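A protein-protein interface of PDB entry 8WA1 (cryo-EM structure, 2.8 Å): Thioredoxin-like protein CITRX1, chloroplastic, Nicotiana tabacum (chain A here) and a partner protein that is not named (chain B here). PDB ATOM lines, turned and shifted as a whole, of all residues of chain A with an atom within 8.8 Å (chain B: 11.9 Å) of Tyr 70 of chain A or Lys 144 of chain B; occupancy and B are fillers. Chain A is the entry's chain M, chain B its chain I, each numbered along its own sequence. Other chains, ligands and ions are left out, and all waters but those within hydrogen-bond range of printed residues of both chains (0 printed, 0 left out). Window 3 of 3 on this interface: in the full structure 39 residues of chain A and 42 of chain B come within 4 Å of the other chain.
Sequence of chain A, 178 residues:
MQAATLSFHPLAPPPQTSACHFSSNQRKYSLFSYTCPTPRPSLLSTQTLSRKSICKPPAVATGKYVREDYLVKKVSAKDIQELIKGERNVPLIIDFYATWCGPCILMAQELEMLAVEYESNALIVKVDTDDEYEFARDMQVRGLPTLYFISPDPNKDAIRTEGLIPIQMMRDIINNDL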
ATOM      1  N   ARG A  67      13.404 -21.897 -26.382  1.00  0.00           N
ATOM      2  CA  ARG A  67      14.736 -21.375 -26.657  1.00  0.00           C
ATOM      3  C   ARG A  67      15.693 -21.744 -25.529  1.00  0.00           C
ATOM      4  O   ARG A  67      15.294 -21.866 -24.368  1.00  0.00           O
ATOM      5  CB  ARG A  67      14.680 -19.857 -26.833  1.00  0.00           C
ATOM      6  CG  ARG A  67      15.982 -19.226 -27.299  1.00  0.00           C
ATOM      7  CD  ARG A  67      16.418 -19.793 -28.640  1.00  0.00           C
ATOM      8  NE  ARG A  67      17.684 -19.222 -29.089  1.00  0.00           N
ATOM      9  CZ  ARG A  67      18.301 -19.567 -30.216  1.00  0.00           C
ATOM     10  NH1 ARG A  67      17.767 -20.483 -31.011  1.00  0.00           N
ATOM     11  NH2 ARG A  67      19.452 -18.996 -30.547  1.00  0.00           N
ATOM     12  N   GLU A  68      16.963 -21.928 -25.879  1.00  0.00           N
ATOM     13  CA  GLU A  68      17.975 -22.246 -24.880  1.00  0.00           C
ATOM     14  C   GLU A  68      18.263 -21.029 -24.009  1.00  0.00           C
ATOM     15  O   GLU A  68      18.333 -19.897 -24.496  1.00  0.00           O
ATOM     16  CB  GLU A  68      19.263 -22.726 -25.552  1.00  0.00           C
ATOM     17  CG  GLU A  68      19.169 -24.110 -26.180  1.00  0.00           C
ATOM     18  CD  GLU A  68      18.395 -24.116 -27.484  1.00  0.00           C
ATOM     19  OE1 GLU A  68      18.132 -23.024 -28.028  1.00  0.00           O
ATOM     20  OE2 GLU A  68      18.048 -25.215 -27.965  1.00  0.00           O
ATOM     21  N   ASP A  69      18.432 -21.270 -22.707  1.00  0.00           N
ATOM     22  CA  ASP A  69      18.660 -20.171 -21.776  1.00  0.00           C
ATOM     23  C   ASP A  69      20.064 -19.599 -21.917  1.00  0.00           C
ATOM     24  O   ASP A  69      20.254 -18.380 -21.845  1.00  0.00           O
ATOM     25  CB  ASP A  69      18.413 -20.644 -20.342  1.00  0.00           C
ATOM     26  CG  ASP A  69      17.009 -21.180 -20.139  1.00  0.00           C
ATOM     27  OD1 ASP A  69      16.216 -21.161 -21.105  1.00  0.00           O
ATOM     28  OD2 ASP A  69      16.697 -21.622 -19.014  1.00  0.00           O
ATOM     29  N   TYR A  70      21.059 -20.459 -22.117  1.00  0.00           N
ATOM     30  CA  TYR A  70      22.455 -20.051 -22.198  1.00  0.00           C
ATOM     31  C   TYR A  70      22.961 -20.254 -23.620  1.00  0.00           C
ATOM     32  O   TYR A  70      22.707 -21.299 -24.231  1.00  0.00           O
ATOM     33  CB  TYR A  70      23.305 -20.842 -21.202  1.00  0.00           C
ATOM     34  CG  TYR A  70      22.781 -20.777 -19.783  1.00  0.00           C
ATOM     35  CD1 TYR A  70      23.163 -19.753 -18.927  1.00  0.00           C
ATOM     36  CD2 TYR A  70      21.899 -21.737 -19.302  1.00  0.00           C
ATOM     37  CE1 TYR A  70      22.683 -19.687 -17.633  1.00  0.00           C
ATOM     38  CE2 TYR A  70      21.415 -21.680 -18.008  1.00  0.00           C
ATOM     39  CZ  TYR A  70      21.811 -20.653 -17.178  1.00  0.00           C
ATOM     40  OH  TYR A  70      21.334 -20.589 -15.889  1.00  0.00           O
ATOM     41  N   LEU A  71      23.674 -19.258 -24.142  1.00  0.00           N
ATOM     42  CA  LEU A  71      24.132 -19.261 -25.525  1.00  0.00           C
ATOM     43  C   LEU A  71      25.621 -19.548 -25.669  1.00  0.00           C
ATOM     44  O   LEU A  71      26.113 -19.635 -26.799  1.00  0.00           O
ATOM     45  CB  LEU A  71      23.804 -17.923 -26.196  1.00  0.00           C
ATOM     46  CG  LEU A  71      22.401 -17.726 -26.778  1.00  0.00           C
ATOM     47  CD1 LEU A  71      21.334 -17.672 -25.692  1.00  0.00           C
ATOM     48  CD2 LEU A  71      22.360 -16.469 -27.634  1.00  0.00           C
ATOM     49  N   VAL A  72      26.349 -19.700 -24.566  1.00  0.00           N
ATOM     50  CA  VAL A  72      27.776 -20.002 -24.597  1.00  0.00           C
ATOM     51  C   VAL A  72      27.959 -21.485 -24.310  1.00  0.00           C
ATOM     52  O   VAL A  72      27.431 -22.002 -23.318  1.00  0.00           O
ATOM     53  CB  VAL A  72      28.551 -19.141 -23.586  1.00  0.00           C
ATOM     54  CG1 VAL A  72      30.007 -19.565 -23.535  1.00  0.00           C
ATOM     55  CG2 VAL A  72      28.438 -17.669 -23.948  1.00  0.00           C
ATOM     56  N   LYS A  73      28.705 -22.168 -25.173  1.00  0.00           N
ATOM     57  CA  LYS A  73      28.893 -23.609 -25.087  1.00  0.00           C
ATOM     58  C   LYS A  73      30.251 -23.936 -24.479  1.00  0.00           C
ATOM     59  O   LYS A  73      31.234 -23.219 -24.687  1.00  0.00           O
ATOM     60  CB  LYS A  73      28.771 -24.261 -26.467  1.00  0.00           C
ATOM     61  CG  LYS A  73      27.478 -23.932 -27.198  1.00  0.00           C
ATOM     62  CD  LYS A  73      26.259 -24.332 -26.382  1.00  0.00           C
ATOM     63  CE  LYS A  73      24.968 -23.966 -27.096  1.00  0.00           C
ATOM     64  NZ  LYS A  73      23.767 -24.318 -26.290  1.00  0.00           N
ATOM     65  N   LYS A  74      30.294 -25.033 -23.726  1.00  0.00           N
ATOM     66  CA  LYS A  74      31.526 -25.500 -23.091  1.00  0.00           C
ATOM     67  C   LYS A  74      32.247 -26.440 -24.048  1.00  0.00           C
ATOM     68  O   LYS A  74      31.843 -27.590 -24.235  1.00  0.00           O
ATOM     69  CB  LYS A  74      31.223 -26.191 -21.767  1.00  0.00           C
ATOM     70  CG  LYS A  74      32.439 -26.830 -21.115  1.00  0.00           C
ATOM     71  CD  LYS A  74      32.052 -27.641 -19.890  1.00  0.00           C
ATOM     72  CE  LYS A  74      33.249 -28.393 -19.331  1.00  0.00           C
ATOM     73  NZ  LYS A  74      32.899 -29.197 -18.129  1.00  0.00           N
ATOM     74  N   TYR A  97      37.053 -20.746 -16.970  1.00  0.00           N
ATOM     75  CA  TYR A  97      36.283 -20.519 -15.793  1.00  0.00           C
ATOM     76  C   TYR A  97      36.360 -21.692 -14.904  1.00  0.00           C
ATOM     77  O   TYR A  97      36.878 -22.711 -15.296  1.00  0.00           O
ATOM     78  CB  TYR A  97      34.834 -20.282 -16.179  1.00  0.00           C
ATOM     79  CG  TYR A  97      34.046 -21.500 -16.584  1.00  0.00           C
ATOM     80  CD1 TYR A  97      34.176 -22.045 -17.842  1.00  0.00           C
ATOM     81  CD2 TYR A  97      33.140 -22.076 -15.715  1.00  0.00           C
ATOM     82  CE1 TYR A  97      33.450 -23.152 -18.213  1.00  0.00           C
ATOM     83  CE2 TYR A  97      32.411 -23.183 -16.079  1.00  0.00           C
ATOM     84  CZ  TYR A  97      32.571 -23.712 -17.331  1.00  0.00           C
ATOM     85  OH  TYR A  97      31.844 -24.813 -17.698  1.00  0.00           O
ATOM     86  N   THR A  99      33.898 -23.480 -11.635  1.00  0.00           N
ATOM     87  CA  THR A  99      32.686 -23.304 -10.904  1.00  0.00           C
ATOM     88  C   THR A  99      33.000 -22.675  -9.571  1.00  0.00           C
ATOM     89  O   THR A  99      32.249 -21.859  -9.078  1.00  0.00           O
ATOM     90  CB  THR A  99      31.947 -24.624 -10.773  1.00  0.00           C
ATOM     91  OG1 THR A  99      32.854 -25.626 -10.308  1.00  0.00           O
ATOM     92  CG2 THR A  99      31.418 -25.052 -12.120  1.00  0.00           C
ATOM     93  N   ILE A 105      31.376 -15.882 -11.643  1.00  0.00           N
ATOM     94  CA  ILE A 105      29.936 -15.830 -11.733  1.00  0.00           C
ATOM     95  C   ILE A 105      29.506 -14.564 -12.439  1.00  0.00           C
ATOM     96  O   ILE A 105      28.564 -14.578 -13.204  1.00  0.00           O
ATOM     97  CB  ILE A 105      29.278 -15.953 -10.362  1.00  0.00           C
ATOM     98  CG1 ILE A 105      29.821 -17.172  -9.628  1.00  0.00           C
ATOM     99  CG2 ILE A 105      27.771 -16.059 -10.489  1.00  0.00           C
ATOM    100  CD1 ILE A 105      29.154 -17.421  -8.298  1.00  0.00           C
ATOM    101  N   ALA A 108      30.643 -14.530 -16.329  1.00  0.00           N
ATOM    102  CA  ALA A 108      29.743 -15.327 -17.157  1.00  0.00           C
ATOM    103  C   ALA A 108      28.525 -14.518 -17.584  1.00  0.00           C
ATOM    104  O   ALA A 108      28.060 -14.638 -18.724  1.00  0.00           O
ATOM    105  CB  ALA A 108      29.314 -16.585 -16.406  1.00  0.00           C
ATOM    106  N   GLN A 109      27.995 -13.685 -16.686  1.00  0.00           N
ATOM    107  CA  GLN A 109      26.853 -12.848 -17.048  1.00  0.00           C
ATOM    108  C   GLN A 109      27.227 -11.842 -18.132  1.00  0.00           C
ATOM    109  O   GLN A 109      26.465 -11.625 -19.083  1.00  0.00           O
ATOM    110  CB  GLN A 109      26.313 -12.130 -15.812  1.00  0.00           C
ATOM    111  CG  GLN A 109      25.697 -13.053 -14.776  1.00  0.00           C
ATOM    112  CD  GLN A 109      25.179 -12.303 -13.567  1.00  0.00           C
ATOM    113  OE1 GLN A 109      25.196 -11.073 -13.531  1.00  0.00           O
ATOM    114  NE2 GLN A 109      24.716 -13.041 -12.567  1.00  0.00           N
ATOM    115  N   GLU A 112      27.511 -13.631 -21.372  1.00  0.00           N
ATOM    116  CA  GLU A 112      26.173 -13.862 -21.910  1.00  0.00           C
ATOM    117  C   GLU A 112      25.634 -12.611 -22.592  1.00  0.00           C
ATOM    118  O   GLU A 112      25.088 -12.683 -23.701  1.00  0.00           O
ATOM    119  CB  GLU A 112      25.228 -14.309 -20.798  1.00  0.00           C
ATOM    120  CG  GLU A 112      25.423 -15.739 -20.330  1.00  0.00           C
ATOM    121  CD  GLU A 112      24.958 -16.754 -21.354  1.00  0.00           C
ATOM    122  OE1 GLU A 112      25.812 -17.312 -22.073  1.00  0.00           O
ATOM    123  OE2 GLU A 112      23.734 -16.985 -21.446  1.00  0.00           O
ATOM    124  N   ALA A 115      27.465 -12.148 -25.866  1.00  0.00           N
ATOM    125  CA  ALA A 115      27.012 -13.105 -26.869  1.00  0.00           C
ATOM    126  C   ALA A 115      25.644 -12.721 -27.414  1.00  0.00           C
ATOM    127  O   ALA A 115      25.355 -12.937 -28.597  1.00  0.00           O
ATOM    128  CB  ALA A 115      26.978 -14.513 -26.274  1.00  0.00           C
ATOM    129  N   VAL A 116      24.782 -12.161 -26.563  1.00  0.00           N
ATOM    130  CA  VAL A 116      23.492 -11.673 -27.043  1.00  0.00           C
ATOM    131  C   VAL A 116      23.687 -10.471 -27.958  1.00  0.00           C
ATOM    132  O   VAL A 116      23.028 -10.351 -28.999  1.00  0.00           O
ATOM    133  CB  VAL A 116      22.565 -11.345 -25.857  1.00  0.00           C
ATOM    134  CG1 VAL A 116      21.281 -10.705 -26.348  1.00  0.00           C
ATOM    135  CG2 VAL A 116      22.251 -12.604 -25.066  1.00  0.00           C
ATOM    136  N   LYS A 126      33.588 -21.223 -23.829  1.00  0.00           N
ATOM    137  CA  LYS A 126      34.127 -21.272 -22.477  1.00  0.00           C
ATOM    138  C   LYS A 126      34.764 -22.631 -22.230  1.00  0.00           C
ATOM    139  O   LYS A 126      34.254 -23.658 -22.685  1.00  0.00           O
ATOM    140  CB  LYS A 126      33.039 -20.996 -21.427  1.00  0.00           C
ATOM    141  CG  LYS A 126      31.866 -21.962 -21.461  1.00  0.00           C
ATOM    142  CD  LYS A 126      30.819 -21.604 -20.419  1.00  0.00           C
ATOM    143  CE  LYS A 126      29.675 -22.605 -20.420  1.00  0.00           C
ATOM    144  NZ  LYS A 126      28.647 -22.286 -19.391  1.00  0.00           N
ATOM    145  N   GLU B 138      35.039 -31.510  -6.867  1.00  0.00           N
ATOM    146  CA  GLU B 138      33.607 -31.274  -6.984  1.00  0.00           C
ATOM    147  C   GLU B 138      33.336 -30.204  -8.034  1.00  0.00           C
ATOM    148  O   GLU B 138      33.956 -29.137  -8.018  1.00  0.00           O
ATOM    149  CB  GLU B 138      33.018 -30.855  -5.637  1.00  0.00           C
ATOM    150  CG  GLU B 138      32.976 -31.966  -4.600  1.00  0.00           C
ATOM    151  CD  GLU B 138      31.875 -32.976  -4.870  1.00  0.00           C
ATOM    152  OE1 GLU B 138      30.920 -32.636  -5.598  1.00  0.00           O
ATOM    153  OE2 GLU B 138      31.964 -34.110  -4.354  1.00  0.00           O
ATOM    154  N   GLN B 139      32.409 -30.496  -8.945  1.00  0.00           N
ATOM    155  CA  GLN B 139      32.032 -29.581 -10.011  1.00  0.00           C
ATOM    156  C   GLN B 139      30.518 -29.440 -10.053  1.00  0.00           C
ATOM    157  O   GLN B 139      29.789 -30.426  -9.903  1.00  0.00           O
ATOM    158  CB  GLN B 139      32.546 -30.066 -11.374  1.00  0.00           C
ATOM    159  CG  GLN B 139      34.053 -30.238 -11.444  1.00  0.00           C
ATOM    160  CD  GLN B 139      34.515 -30.785 -12.783  1.00  0.00           C
ATOM    161  OE1 GLN B 139      35.705 -31.014 -12.995  1.00  0.00           O
ATOM    162  NE2 GLN B 139      33.572 -30.996 -13.693  1.00  0.00           N
ATOM    163  N   MET B 140      30.051 -28.214 -10.259  1.00  0.00           N
ATOM    164  CA  MET B 140      28.631 -27.919 -10.380  1.00  0.00           C
ATOM    165  C   MET B 140      28.227 -27.850 -11.850  1.00  0.00           C
ATOM    166  O   MET B 140      28.999 -28.187 -12.751  1.00  0.00           O
ATOM    167  CB  MET B 140      28.293 -26.608  -9.666  1.00  0.00           C
ATOM    168  CG  MET B 140      28.453 -26.676  -8.156  1.00  0.00           C
ATOM    169  SD  MET B 140      27.468 -27.998  -7.427  1.00  0.00           S
ATOM    170  CE  MET B 140      28.014 -27.923  -5.723  1.00  0.00           C
ATOM    171  N   HIS B 141      26.987 -27.420 -12.079  1.00  0.00           N
ATOM    172  CA  HIS B 141      26.468 -27.317 -13.436  1.00  0.00           C
ATOM    173  C   HIS B 141      27.303 -26.339 -14.254  1.00  0.00           C
ATOM    174  O   HIS B 141      27.711 -25.283 -13.766  1.00  0.00           O
ATOM    175  CB  HIS B 141      25.003 -26.878 -13.416  1.00  0.00           C
ATOM    176  CG  HIS B 141      24.282 -27.128 -14.704  1.00  0.00           C
ATOM    177  ND1 HIS B 141      24.331 -26.251 -15.766  1.00  0.00           N
ATOM    178  CD2 HIS B 141      23.497 -28.157 -15.102  1.00  0.00           C
ATOM    179  CE1 HIS B 141      23.608 -26.729 -16.762  1.00  0.00           C
ATOM    180  NE2 HIS B 141      23.090 -27.884 -16.385  1.00  0.00           N
ATOM    181  N   GLN B 142      27.559 -26.709 -15.511  1.00  0.00           N
ATOM    182  CA  GLN B 142      28.424 -25.902 -16.364  1.00  0.00           C
ATOM    183  C   GLN B 142      27.792 -24.558 -16.707  1.00  0.00           C
ATOM    184  O   GLN B 142      28.477 -23.529 -16.728  1.00  0.00           O
ATOM    185  CB  GLN B 142      28.759 -26.675 -17.640  1.00  0.00           C
ATOM    186  CG  GLN B 142      27.592 -27.472 -18.193  1.00  0.00           C
ATOM    187  CD  GLN B 142      27.881 -28.056 -19.559  1.00  0.00           C
ATOM    188  OE1 GLN B 142      27.803 -29.267 -19.757  1.00  0.00           O
ATOM    189  NE2 GLN B 142      28.208 -27.193 -20.512  1.00  0.00           N
ATOM    190  N   ASP B 143      26.485 -24.545 -16.977  1.00  0.00           N
ATOM    191  CA  ASP B 143      25.808 -23.338 -17.430  1.00  0.00           C
ATOM    192  C   ASP B 143      25.069 -22.589 -16.331  1.00  0.00           C
ATOM    193  O   ASP B 143      25.030 -21.356 -16.371  1.00  0.00           O
ATOM    194  CB  ASP B 143      24.812 -23.674 -18.549  1.00  0.00           C
ATOM    195  CG  ASP B 143      25.479 -24.310 -19.753  1.00  0.00           C
ATOM    196  OD1 ASP B 143      26.648 -23.970 -20.033  1.00  0.00           O
ATOM    197  OD2 ASP B 143      24.836 -25.150 -20.415  1.00  0.00           O
ATOM    198  N   LYS B 144      24.503 -23.287 -15.351  1.00  0.00           N
ATOM    199  CA  LYS B 144      23.721 -22.638 -14.303  1.00  0.00           C
ATOM    200  C   LYS B 144      24.670 -22.062 -13.260  1.00  0.00           C
ATOM    201  O   LYS B 144      25.223 -22.798 -12.437  1.00  0.00           O
ATOM    202  CB  LYS B 144      22.749 -23.628 -13.666  1.00  0.00           C
ATOM    203  CG  LYS B 144      21.767 -24.264 -14.635  1.00  0.00           C
ATOM    204  CD  LYS B 144      20.847 -25.240 -13.917  1.00  0.00           C
ATOM    205  CE  LYS B 144      19.879 -25.902 -14.881  1.00  0.00           C
ATOM    206  NZ  LYS B 144      18.976 -26.861 -14.187  1.00  0.00           N
ATOM    207  N   TYR B 145      24.855 -20.744 -13.286  1.00  0.00           N
ATOM    208  CA  TYR B 145      25.696 -20.063 -12.314  1.00  0.00           C
ATOM    209  C   TYR B 145      24.946 -19.705 -11.039  1.00  0.00           C
ATOM    210  O   TYR B 145      25.503 -19.014 -10.179  1.00  0.00           O
ATOM    211  CB  TYR B 145      26.310 -18.801 -12.931  1.00  0.00           C
ATOM    212  CG  TYR B 145      25.317 -17.912 -13.644  1.00  0.00           C
ATOM    213  CD1 TYR B 145      24.525 -17.016 -12.938  1.00  0.00           C
ATOM    214  CD2 TYR B 145      25.179 -17.962 -15.024  1.00  0.00           C
ATOM    215  CE1 TYR B 145      23.619 -16.202 -13.587  1.00  0.00           C
ATOM    216  CE2 TYR B 145      24.278 -17.151 -15.680  1.00  0.00           C
ATOM    217  CZ  TYR B 145      23.499 -16.273 -14.958  1.00  0.00           C
ATOM    218  OH  TYR B 145      22.598 -15.462 -15.607  1.00  0.00           O
ATOM    219  N   SER B 146      23.704 -20.159 -10.895  1.00  0.00           N
ATOM    220  CA  SER B 146      22.940 -19.965  -9.671  1.00  0.00           C
ATOM    221  C   SER B 146      23.126 -21.108  -8.686  1.00  0.00           C
ATOM    222  O   SER B 146      22.625 -21.027  -7.561  1.00  0.00           O
ATOM    223  CB  SER B 146      21.454 -19.793  -9.996  1.00  0.00           C
ATOM    224  OG  SER B 146      20.941 -20.935 -10.657  1.00  0.00           O
ATOM    225  N   GLU B 147      23.834 -22.165  -9.081  1.00  0.00           N
ATOM    226  CA  GLU B 147      24.154 -23.280  -8.202  1.00  0.00           C
ATOM    227  C   GLU B 147      25.621 -23.287  -7.795  1.00  0.00           C
ATOM    228  O   GLU B 147      26.052 -24.194  -7.076  1.00  0.00           O
ATOM    229  CB  GLU B 147      23.793 -24.607  -8.875  1.00  0.00           C
ATOM    230  CG  GLU B 147      22.342 -24.714  -9.304  1.00  0.00           C
ATOM    231  CD  GLU B 147      22.042 -26.019 -10.014  1.00  0.00           C
ATOM    232  OE1 GLU B 147      22.972 -26.837 -10.174  1.00  0.00           O
ATOM    233  OE2 GLU B 147      20.877 -26.226 -10.413  1.00  0.00           O
ATOM    234  N   TRP B 148      26.396 -22.298  -8.235  1.00  0.00           N
ATOM    235  CA  TRP B 148      27.808 -22.214  -7.893  1.00  0.00           C
ATOM    236  C   TRP B 148      28.046 -21.665  -6.493  1.00  0.00           C
ATOM    237  O   TRP B 148      29.170 -21.766  -5.988  1.00  0.00           O
ATOM    238  CB  TRP B 148      28.550 -21.346  -8.915  1.00  0.00           C
ATOM    239  CG  TRP B 148      28.556 -21.912 -10.307  1.00  0.00           C
ATOM    240  CD1 TRP B 148      28.041 -23.109 -10.710  1.00  0.00           C
ATOM    241  CD2 TRP B 148      29.104 -21.296 -11.480  1.00  0.00           C
ATOM    242  NE1 TRP B 148      28.235 -23.278 -12.060  1.00  0.00           N
ATOM    243  CE2 TRP B 148      28.885 -22.179 -12.556  1.00  0.00           C
ATOM    244  CE3 TRP B 148      29.759 -20.085 -11.723  1.00  0.00           C
ATOM    245  CZ2 TRP B 148      29.297 -21.889 -13.854  1.00  0.00           C
ATOM    246  CZ3 TRP B 148      30.166 -19.799 -13.012  1.00  0.00           C
ATOM    247  CH2 TRP B 148      29.935 -20.697 -14.061  1.00  0.00           C
ATOM    248  N   LYS B 149      27.022 -21.093  -5.856  1.00  0.00           N
ATOM    249  CA  LYS B 149      27.162 -20.651  -4.475  1.00  0.00           C
ATOM    250  C   LYS B 149      27.248 -21.824  -3.509  1.00  0.00           C
ATOM    251  O   LYS B 149      27.741 -21.654  -2.390  1.00  0.00           O
ATOM    252  CB  LYS B 149      25.999 -19.736  -4.089  1.00  0.00           C
ATOM    253  CG  LYS B 149      24.640 -20.413  -4.103  1.00  0.00           C
ATOM    254  CD  LYS B 149      23.530 -19.423  -3.795  1.00  0.00           C
ATOM    255  CE  LYS B 149      23.427 -18.359  -4.875  1.00  0.00           C
ATOM    256  NZ  LYS B 149      22.335 -17.386  -4.598  1.00  0.00           N
ATOM    257  N   MET B 150      26.779 -23.007  -3.914  1.00  0.00           N
ATOM    258  CA  MET B 150      26.936 -24.199  -3.092  1.00  0.00           C
ATOM    259  C   MET B 150      28.394 -24.596  -2.920  1.00  0.00           C
ATOM    260  O   MET B 150      28.721 -25.276  -1.941  1.00  0.00           O
ATOM    261  CB  MET B 150      26.149 -25.363  -3.696  1.00  0.00           C
ATOM    262  CG  MET B 150      24.651 -25.118  -3.779  1.00  0.00           C
ATOM    263  SD  MET B 150      23.755 -26.517  -4.478  1.00  0.00           S
ATOM    264  CE  MET B 150      24.165 -27.802  -3.301  1.00  0.00           C
ATOM    265  N   LEU B 151      29.255 -24.050  -3.761  1.00  0.00           N
ATOM    266  CA  LEU B 151      30.676 -24.350  -3.674  1.00  0.00           C
ATOM    267  C   LEU B 151      31.370 -23.307  -2.876  1.00  0.00           C
ATOM    268  O   LEU B 151      32.467 -23.517  -2.440  1.00  0.00           O
ATOM    269  CB  LEU B 151      31.296 -24.475  -5.042  1.00  0.00           C
ATOM    270  CG  LEU B 151      32.201 -25.677  -5.285  1.00  0.00           C
ATOM    271  CD1 LEU B 151      31.671 -26.903  -4.569  1.00  0.00           C
ATOM    272  CD2 LEU B 151      32.328 -25.943  -6.771  1.00  0.00           C
ATOM    273  N   GLN B 152      30.793 -22.137  -2.740  1.00  0.00           N
ATOM    274  CA  GLN B 152      31.346 -21.151  -1.842  1.00  0.00           C
ATOM    275  C   GLN B 152      31.116 -21.675  -0.458  1.00  0.00           C
ATOM    276  O   GLN B 152      31.930 -21.498   0.410  1.00  0.00           O
ATOM    277  CB  GLN B 152      30.677 -19.817  -2.016  1.00  0.00           C
ATOM    278  CG  GLN B 152      30.815 -19.234  -3.402  1.00  0.00           C
ATOM    279  CD  GLN B 152      32.215 -18.758  -3.685  1.00  0.00           C
ATOM    280  OE1 GLN B 152      32.892 -18.240  -2.808  1.00  0.00           O
ATOM    281  NE2 GLN B 152      32.653 -18.921  -4.920  1.00  0.00           N
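O of Gln 142 of chain B is in hydrogen-bond range of NZ of Lys 126 of chain A, 2.9 Å away.
The side-chain amino group (NZ) of Lys 126 of chain A is in salt-bridge range of the side-chain carboxylate (OD1) of Asp 143 of chain B (2.7 Å).
Among the printed residues, merely in contact across the chains: Tyr 70 of chain A with Asp 143 of chain B (3.1 Å), Tyr 70 of chain A with Lys 144 of chain B (3.5 Å), Tyr 70 of chain A with Tyr 145 of chain B (3.6 Å), Val 72 of chain A with Asp 143 of chain B (3.9 Å), Lys 74 of chain A with Gln 142 of chain B (3.4 Å), Tyr 97 of chain A with Gln 142 of chain B (3.6 Å), Tyr 97 of chain A with Trp 148 of chain B (3.9 Å), Thr 99 of chain A with Met 140 of chain B (3.8 Å), Thr 99 of chain A with Trp 148 of chain B (3.6 Å), Thr 99 of chain A with Leu 151 of chain B (3.6 Å), Ile 105 of chain A with Tyr 145 of chain B (3.7 Å), Ile 105 of chain A with Trp 148 of chain B (3.6 Å) and Gln 109 of chain A with Tyr 145 of chain B (3.5 Å).
Printed residues of chain B within 4 Å of Tyr 70 of chain A: Asp 143 (3.1 Å), Lys 144 (3.5 Å) and Tyr 145 (3.6 Å).
Lys 144 of chain B touches just one residue of chain A: Tyr 70.
No residue of chain B comes within 4 Å of Glu 68 of chain A.
No residue of chain B comes within 4 Å of Asp 69 of chain A.
No residue of chain B comes within 4 Å of Leu 71 of chain A.
Val 72 of chain A touches just one residue of chain B: Asp 143.
Of chain A, only Tyr 70 (3.1 Å), Val 72 (3.9 Å) and Lys 126 (2.7 Å) come within 4 Å of Asp 143 of chain B.
Of the printed residues of chain A, Leu 151 of chain B touches Thr 99 (3.6 Å).
Printed residues of chain A within 4 Å of Tyr 145 of chain B: Tyr 70 (3.6 Å), Ile 105 (3.7 Å) and Gln 109 (3.5 Å).
The nearest residue of chain A that does not touch Lys 144 of chain B is Lys 126 of chain A (5.9 Å).
Of the 17 printed residues of chain A, 8 touch a printed residue of chain B.
Hydrophobic or aromatic side chains of chain A within 4 Å of the printed part of chain B: Tyr 70, Tyr 97 and Ile 105.
Of the 15 printed residues of chain B, 7 touch a printed residue of chain A.
Printed residues of chain B that touch a printed residue of chain A: Met 140, Gln 142, Asp 143, Lys 144, Tyr 145, Trp 148 and Leu 151.
Hydrophobic or aromatic side chains of chain B that line the printed part of chain A: Tyr 145, Trp 148 and Leu 151.
Among the printed residues, 15 pairs touch across the chains.
The side-chain carboxylate (OE1) of Glu 112 of chain A lies close to the backbone NH (N) of Val 72 of chain A, 3.5 Å away.
The backbone carbonyl oxygen (O) of Lys 73 of chain A is in hydrogen-bond range of the backbone NH (N) of Lys 126 of chain A, at 3.2 Å.
A ring nitrogen (ND1) of His 141 of chain B sits at hydrogen-bond distance from the backbone NH of Asp 143 of chain B, 3.0 Å away.
ND1 of His 141 of chain B is in hydrogen-bond range of N of Lys 144 of chain B (3.0 Å).
O of His 141 of chain B lies within hydrogen-bond range of NE1 of Trp 148 of chain B (2.7 Å).
O of Lys 144 of chain B sits at hydrogen-bond distance from NE1 of Trp 148 of chain B.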
